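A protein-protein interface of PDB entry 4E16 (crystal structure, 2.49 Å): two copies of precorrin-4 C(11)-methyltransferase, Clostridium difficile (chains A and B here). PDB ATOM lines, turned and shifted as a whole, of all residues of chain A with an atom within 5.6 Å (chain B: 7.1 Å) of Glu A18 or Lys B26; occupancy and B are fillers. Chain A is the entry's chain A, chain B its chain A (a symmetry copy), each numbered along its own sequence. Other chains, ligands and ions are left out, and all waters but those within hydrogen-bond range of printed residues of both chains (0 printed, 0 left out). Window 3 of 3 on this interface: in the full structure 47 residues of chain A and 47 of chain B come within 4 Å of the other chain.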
ATOM      1  N   ASP A  16     -32.120  32.787   2.730  1.00  0.00           N
ATOM      2  CA  ASP A  16     -31.332  31.591   2.388  1.00  0.00           C
ATOM      3  C   ASP A  16     -29.810  31.881   2.338  1.00  0.00           C
ATOM      4  O   ASP A  16     -29.350  32.799   1.659  1.00  0.00           O
ATOM      5  CB  ASP A  16     -31.851  30.999   1.076  1.00  0.00           C
ATOM      6  CG  ASP A  16     -31.245  29.642   0.726  1.00  0.00           C
ATOM      7  OD1 ASP A  16     -31.884  28.936  -0.057  1.00  0.00           O
ATOM      8  OD2 ASP A  16     -30.135  29.288   1.137  1.00  0.00           O
ATOM      9  N   LYS A  17     -29.103  31.110   3.152  1.00  0.00           N
ATOM     10  CA  LYS A  17     -27.655  31.032   3.284  1.00  0.00           C
ATOM     11  C   LYS A  17     -26.989  31.320   1.915  1.00  0.00           C
ATOM     12  O   LYS A  17     -26.199  32.245   1.748  1.00  0.00           O
ATOM     13  CB  LYS A  17     -27.338  29.587   3.775  1.00  0.00           C
ATOM     14  CG  LYS A  17     -26.065  29.457   4.554  1.00  0.00           C
ATOM     15  CD  LYS A  17     -25.469  28.065   4.440  1.00  0.00           C
ATOM     16  CE  LYS A  17     -26.042  27.044   5.411  1.00  0.00           C
ATOM     17  NZ  LYS A  17     -26.045  25.700   4.745  1.00  0.00           N
ATOM     18  N   GLU A  18     -27.396  30.541   0.928  1.00  0.00           N
ATOM     19  CA  GLU A  18     -26.795  30.476  -0.391  1.00  0.00           C
ATOM     20  C   GLU A  18     -27.236  31.542  -1.363  1.00  0.00           C
ATOM     21  O   GLU A  18     -26.761  31.590  -2.488  1.00  0.00           O
ATOM     22  CB  GLU A  18     -27.184  29.155  -0.965  1.00  0.00           C
ATOM     23  CG  GLU A  18     -26.886  27.997  -0.025  1.00  0.00           C
ATOM     24  CD  GLU A  18     -26.354  26.802  -0.778  1.00  0.00           C
ATOM     25  OE1 GLU A  18     -27.066  26.229  -1.658  1.00  0.00           O
ATOM     26  OE2 GLU A  18     -25.207  26.457  -0.480  1.00  0.00           O
ATOM     27  N   LEU A  19     -28.169  32.391  -0.957  1.00  0.00           N
ATOM     28  CA  LEU A  19     -28.592  33.467  -1.815  1.00  0.00           C
ATOM     29  C   LEU A  19     -27.791  34.718  -1.596  1.00  0.00           C
ATOM     30  O   LEU A  19     -28.170  35.778  -2.123  1.00  0.00           O
ATOM     31  CB  LEU A  19     -30.051  33.785  -1.593  1.00  0.00           C
ATOM     32  CG  LEU A  19     -30.971  32.668  -2.053  1.00  0.00           C
ATOM     33  CD1 LEU A  19     -32.413  33.121  -1.820  1.00  0.00           C
ATOM     34  CD2 LEU A  19     -30.682  32.192  -3.499  1.00  0.00           C
ATOM     35  N   ILE A  20     -26.723  34.641  -0.792  1.00  0.00           N
ATOM     36  CA  ILE A  20     -25.792  35.760  -0.788  1.00  0.00           C
ATOM     37  C   ILE A  20     -25.103  35.706  -2.136  1.00  0.00           C
ATOM     38  O   ILE A  20     -25.011  34.611  -2.721  1.00  0.00           O
ATOM     39  CB  ILE A  20     -24.776  35.748   0.367  1.00  0.00           C
ATOM     40  CG1 ILE A  20     -24.182  37.164   0.494  1.00  0.00           C
ATOM     41  CG2 ILE A  20     -23.662  34.698   0.186  1.00  0.00           C
ATOM     42  CD1 ILE A  20     -23.280  37.381   1.706  1.00  0.00           C
ATOM     43  N   LEU A  45     -25.636  32.396   7.933  1.00  0.00           N
ATOM     44  CA  LEU A  45     -24.596  33.152   7.170  1.00  0.00           C
ATOM     45  C   LEU A  45     -23.275  33.337   7.902  1.00  0.00           C
ATOM     46  O   LEU A  45     -22.209  33.277   7.299  1.00  0.00           O
ATOM     47  CB  LEU A  45     -25.067  34.561   6.812  1.00  0.00           C
ATOM     48  CG  LEU A  45     -26.048  34.707   5.679  1.00  0.00           C
ATOM     49  CD1 LEU A  45     -26.529  36.159   5.532  1.00  0.00           C
ATOM     50  CD2 LEU A  45     -25.414  34.215   4.386  1.00  0.00           C
ATOM     51  N   TYR A  48     -20.059  31.224   7.617  1.00  0.00           N
ATOM     52  CA  TYR A  48     -19.100  31.434   6.547  1.00  0.00           C
ATOM     53  C   TYR A  48     -17.853  32.229   7.021  1.00  0.00           C
ATOM     54  O   TYR A  48     -16.827  32.231   6.345  1.00  0.00           O
ATOM     55  CB  TYR A  48     -19.749  32.203   5.415  1.00  0.00           C
ATOM     56  CG  TYR A  48     -20.847  31.522   4.612  1.00  0.00           C
ATOM     57  CD1 TYR A  48     -20.728  30.208   4.132  1.00  0.00           C
ATOM     58  CD2 TYR A  48     -21.975  32.248   4.237  1.00  0.00           C
ATOM     59  CE1 TYR A  48     -21.725  29.624   3.356  1.00  0.00           C
ATOM     60  CE2 TYR A  48     -22.977  31.683   3.462  1.00  0.00           C
ATOM     61  CZ  TYR A  48     -22.858  30.374   3.025  1.00  0.00           C
ATOM     62  OH  TYR A  48     -23.903  29.868   2.265  1.00  0.00           O
ATOM     63  N   ILE B  20     -23.410  36.913  -9.192  1.00  0.00           N
ATOM     64  CA  ILE B  20     -24.296  35.758  -9.188  1.00  0.00           C
ATOM     65  C   ILE B  20     -24.397  35.341  -7.735  1.00  0.00           C
ATOM     66  O   ILE B  20     -23.455  35.611  -6.966  1.00  0.00           O
ATOM     67  CB  ILE B  20     -23.838  34.591 -10.080  1.00  0.00           C
ATOM     68  CG1 ILE B  20     -25.048  33.668 -10.317  1.00  0.00           C
ATOM     69  CG2 ILE B  20     -22.651  33.804  -9.489  1.00  0.00           C
ATOM     70  CD1 ILE B  20     -24.819  32.548 -11.328  1.00  0.00           C
ATOM     71  N   THR B  21     -25.539  34.773  -7.341  1.00  0.00           N
ATOM     72  CA  THR B  21     -25.639  34.129  -6.023  1.00  0.00           C
ATOM     73  C   THR B  21     -24.663  32.952  -5.840  1.00  0.00           C
ATOM     74  O   THR B  21     -24.312  32.230  -6.770  1.00  0.00           O
ATOM     75  CB  THR B  21     -27.046  33.579  -5.714  1.00  0.00           C
ATOM     76  OG1 THR B  21     -27.437  32.646  -6.715  1.00  0.00           O
ATOM     77  CG2 THR B  21     -28.055  34.705  -5.679  1.00  0.00           C
ATOM     78  N   LEU B  22     -24.220  32.764  -4.622  1.00  0.00           N
ATOM     79  CA  LEU B  22     -23.539  31.529  -4.261  1.00  0.00           C
ATOM     80  C   LEU B  22     -24.256  30.322  -4.830  1.00  0.00           C
ATOM     81  O   LEU B  22     -23.617  29.557  -5.512  1.00  0.00           O
ATOM     82  CB  LEU B  22     -23.455  31.426  -2.738  1.00  0.00           C
ATOM     83  CG  LEU B  22     -22.429  30.468  -2.168  1.00  0.00           C
ATOM     84  CD1 LEU B  22     -21.114  30.477  -2.961  1.00  0.00           C
ATOM     85  CD2 LEU B  22     -22.232  30.920  -0.753  1.00  0.00           C
ATOM     86  N   LYS B  23     -25.579  30.189  -4.624  1.00  0.00           N
ATOM     87  CA  LYS B  23     -26.354  29.021  -5.121  1.00  0.00           C
ATOM     88  C   LYS B  23     -26.265  28.884  -6.638  1.00  0.00           C
ATOM     89  O   LYS B  23     -26.049  27.786  -7.221  1.00  0.00           O
ATOM     90  CB  LYS B  23     -27.821  29.115  -4.748  1.00  0.00           C
ATOM     91  CG  LYS B  23     -28.554  27.791  -4.951  1.00  0.00           C
ATOM     92  CD  LYS B  23     -29.999  27.839  -4.427  1.00  0.00           C
ATOM     93  CE  LYS B  23     -30.106  27.556  -2.915  1.00  0.00           C
ATOM     94  NZ  LYS B  23     -31.381  28.096  -2.360  1.00  0.00           N
ATOM     95  N   GLY B  24     -26.414  30.029  -7.276  1.00  0.00           N
ATOM     96  CA  GLY B  24     -26.236  30.117  -8.700  1.00  0.00           C
ATOM     97  C   GLY B  24     -24.886  29.623  -9.141  1.00  0.00           C
ATOM     98  O   GLY B  24     -24.796  28.786 -10.050  1.00  0.00           O
ATOM     99  N   TYR B  25     -23.840  30.126  -8.500  1.00  0.00           N
ATOM    100  CA  TYR B  25     -22.493  29.704  -8.824  1.00  0.00           C
ATOM    101  C   TYR B  25     -22.285  28.162  -8.705  1.00  0.00           C
ATOM    102  O   TYR B  25     -21.685  27.557  -9.615  1.00  0.00           O
ATOM    103  CB  TYR B  25     -21.489  30.461  -7.963  1.00  0.00           C
ATOM    104  CG  TYR B  25     -20.121  29.918  -8.039  1.00  0.00           C
ATOM    105  CD1 TYR B  25     -19.573  29.213  -6.978  1.00  0.00           C
ATOM    106  CD2 TYR B  25     -19.391  30.065  -9.183  1.00  0.00           C
ATOM    107  CE1 TYR B  25     -18.274  28.710  -7.038  1.00  0.00           C
ATOM    108  CE2 TYR B  25     -18.121  29.557  -9.287  1.00  0.00           C
ATOM    109  CZ  TYR B  25     -17.559  28.896  -8.207  1.00  0.00           C
ATOM    110  OH  TYR B  25     -16.295  28.408  -8.360  1.00  0.00           O
ATOM    111  N   LYS B  26     -22.795  27.541  -7.626  1.00  0.00           N
ATOM    112  CA  LYS B  26     -22.648  26.076  -7.437  1.00  0.00           C
ATOM    113  C   LYS B  26     -23.277  25.302  -8.574  1.00  0.00           C
ATOM    114  O   LYS B  26     -22.679  24.372  -9.115  1.00  0.00           O
ATOM    115  CB  LYS B  26     -23.286  25.606  -6.133  1.00  0.00           C
ATOM    116  CG  LYS B  26     -22.603  26.170  -4.902  1.00  0.00           C
ATOM    117  CD  LYS B  26     -23.024  25.356  -3.695  1.00  0.00           C
ATOM    118  CE  LYS B  26     -22.481  25.880  -2.375  1.00  0.00           C
ATOM    119  NZ  LYS B  26     -22.086  24.728  -1.491  1.00  0.00           N
ATOM    120  N   LEU B  27     -24.490  25.711  -8.947  1.00  0.00           N
ATOM    121  CA  LEU B  27     -25.243  25.041  -9.986  1.00  0.00           C
ATOM    122  C   LEU B  27     -24.557  25.249 -11.283  1.00  0.00           C
ATOM    123  O   LEU B  27     -24.384  24.305 -12.057  1.00  0.00           O
ATOM    124  CB  LEU B  27     -26.667  25.572 -10.056  1.00  0.00           C
ATOM    125  CG  LEU B  27     -27.621  25.109  -8.943  1.00  0.00           C
ATOM    126  CD1 LEU B  27     -28.837  26.034  -9.009  1.00  0.00           C
ATOM    127  CD2 LEU B  27     -28.003  23.610  -9.019  1.00  0.00           C
ATOM    128  N   LEU B  28     -24.128  26.478 -11.525  1.00  0.00           N
ATOM    129  CA  LEU B  28     -23.441  26.745 -12.805  1.00  0.00           C
ATOM    130  C   LEU B  28     -22.114  25.997 -12.921  1.00  0.00           C
ATOM    131  O   LEU B  28     -21.750  25.493 -14.010  1.00  0.00           O
ATOM    132  CB  LEU B  28     -23.140  28.229 -12.961  1.00  0.00           C
ATOM    133  CG  LEU B  28     -23.502  29.064 -14.165  1.00  0.00           C
ATOM    134  CD1 LEU B  28     -22.347  30.058 -14.306  1.00  0.00           C
ATOM    135  CD2 LEU B  28     -23.726  28.204 -15.408  1.00  0.00           C
ATOM    136  N   SER B  29     -21.370  25.967 -11.822  1.00  0.00           N
ATOM    137  CA  SER B  29     -20.034  25.430 -11.924  1.00  0.00           C
ATOM    138  C   SER B  29     -20.083  23.901 -12.022  1.00  0.00           C
ATOM    139  O   SER B  29     -19.081  23.287 -12.398  1.00  0.00           O
ATOM    140  CB  SER B  29     -19.095  25.941 -10.817  1.00  0.00           C
ATOM    141  OG  SER B  29     -19.620  25.584  -9.580  1.00  0.00           O
ATOM    142  N   ASN B  30     -21.267  23.331 -11.764  1.00  0.00           N
ATOM    143  CA  ASN B  30     -21.536  21.870 -11.875  1.00  0.00           C
ATOM    144  C   ASN B  30     -22.408  21.397 -13.062  1.00  0.00           C
ATOM    145  O   ASN B  30     -22.678  20.211 -13.229  1.00  0.00           O
ATOM    146  CB  ASN B  30     -22.179  21.404 -10.596  1.00  0.00           C
ATOM    147  CG  ASN B  30     -21.200  21.399  -9.460  1.00  0.00           C
ATOM    148  OD1 ASN B  30     -20.263  20.595  -9.468  1.00  0.00           O
ATOM    149  ND2 ASN B  30     -21.369  22.320  -8.490  1.00  0.00           N
ATOM    150  N   ALA B  31     -22.841  22.336 -13.886  1.00  0.00           N
ATOM    151  CA  ALA B  31     -23.780  22.064 -14.933  1.00  0.00           C
ATOM    152  C   ALA B  31     -23.122  21.325 -16.073  1.00  0.00           C
ATOM    153  O   ALA B  31     -21.969  21.617 -16.433  1.00  0.00           O
ATOM    154  CB  ALA B  31     -24.356  23.365 -15.421  1.00  0.00           C
ATOM    155  N   VAL B  81     -28.774  23.870 -16.621  1.00  0.00           N
ATOM    156  CA  VAL B  81     -28.962  25.222 -16.114  1.00  0.00           C
ATOM    157  C   VAL B  81     -29.290  26.204 -17.241  1.00  0.00           C
ATOM    158  O   VAL B  81     -28.501  26.315 -18.199  1.00  0.00           O
ATOM    159  CB  VAL B  81     -27.691  25.768 -15.432  1.00  0.00           C
ATOM    160  CG1 VAL B  81     -27.874  27.252 -15.208  1.00  0.00           C
ATOM    161  CG2 VAL B  81     -27.399  25.076 -14.098  1.00  0.00           C
ATOM    162  N   THR B 111     -33.964  29.917  -9.150  1.00  0.00           N
ATOM    163  CA  THR B 111     -32.958  30.480  -8.212  1.00  0.00           C
ATOM    164  C   THR B 111     -32.867  31.959  -8.544  1.00  0.00           C
ATOM    165  O   THR B 111     -32.346  32.316  -9.568  1.00  0.00           O
ATOM    166  CB  THR B 111     -31.553  29.839  -8.401  1.00  0.00           C
ATOM    167  OG1 THR B 111     -31.509  28.571  -7.768  1.00  0.00           O
ATOM    168  CG2 THR B 111     -30.438  30.684  -7.805  1.00  0.00           C
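OD1 of Asp A16 lies within salt-bridge range of NZ of Lys B23, 2.5 Å away.
N of Lys B23 sits at hydrogen-bond distance from O of Glu A18 (2.8 Å).
NZ of Lys B26 is in salt-bridge range of OE2 of Glu A18.
O of Ile A20 lies within hydrogen-bond range of N of Leu B22, 2.8 Å away.
Among the printed residues, merely in contact across the chains: Glu A18 with Thr B21, Glu A18 with Leu B22, Leu A19 with Thr B21, Ile A20 with Thr B21 and Tyr A48 with Leu B22.
Printed residues of chain B within 4 Å of Asp A16: Lys B23 (2.5 Å).
Printed residues of chain B within 4 Å of Leu A19: Thr B21 (3.7 Å).
Printed residues of chain B within 4 Å of Tyr A48: Leu B22.
Of the printed residues of chain A, Thr B21 touches Glu A18 (3.8 Å), Leu A19 (3.7 Å) and Ile A20 (3.4 Å).
Of the printed residues of chain A, Leu B22 touches Glu A18, Ile A20 and Tyr A48.
Tyr B25 touches none of the printed residues of chain A.
Lys B26 touches one residue of chain A.
The nearest residue of chain B that does not touch Glu A18 is Gly B24 (5.0 Å).
The nearest printed residue of chain A that does not touch Lys B26 is Tyr A48 (6.3 Å).
1 position is printed for both chains.
Of the 9 pairs that touch across the chains among the printed residues, none has its exchanged pair printed and touching as well.
OD2 of Asp A16 sits at hydrogen-bond distance from N of Glu A18 (3.0 Å).
The backbone carbonyl oxygen (O) of Lys A17 sits close to the side-chain hydroxyl (OH) of Tyr A48 (3.3 Å).
The backbone NH of Gly B24 sits at hydrogen-bond distance from the side-chain hydroxyl of Thr B21, at 2.9 Å.
The backbone carbonyl oxygen (O) of Lys B26 sits at hydrogen-bond distance from the side-chain hydroxyl (OG) of Ser B29 (3.3 Å).
The backbone carbonyl oxygen (O) of Lys B26 sits at hydrogen-bond distance from the side-chain amide nitrogen (ND2) of Asn B30 (2.5 Å).
Printed residues of chain B that touch a printed residue of chain A: Thr B21, Leu B22, Lys B23 and Lys B26.
Along chain B the printed residues that touch a printed residue of chain A span positions 21 to 26.
Of the 7 printed residues of chain A, 5 touch a printed residue of chain B.
Printed residues of chain A that touch a printed residue of chain B: Asp A16, Glu A18, Leu A19, Ile A20 and Tyr A48.
Among the printed residues, 9 pairs touch across the chains.
Among the printed residues, Asp or Glu carboxylates within 4 Å of a Lys or Arg side-chain nitrogen of the other chain: Asp A16 with Lys B23 (2.5 Å) and Glu A18 with Lys B26 (3.7 Å).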
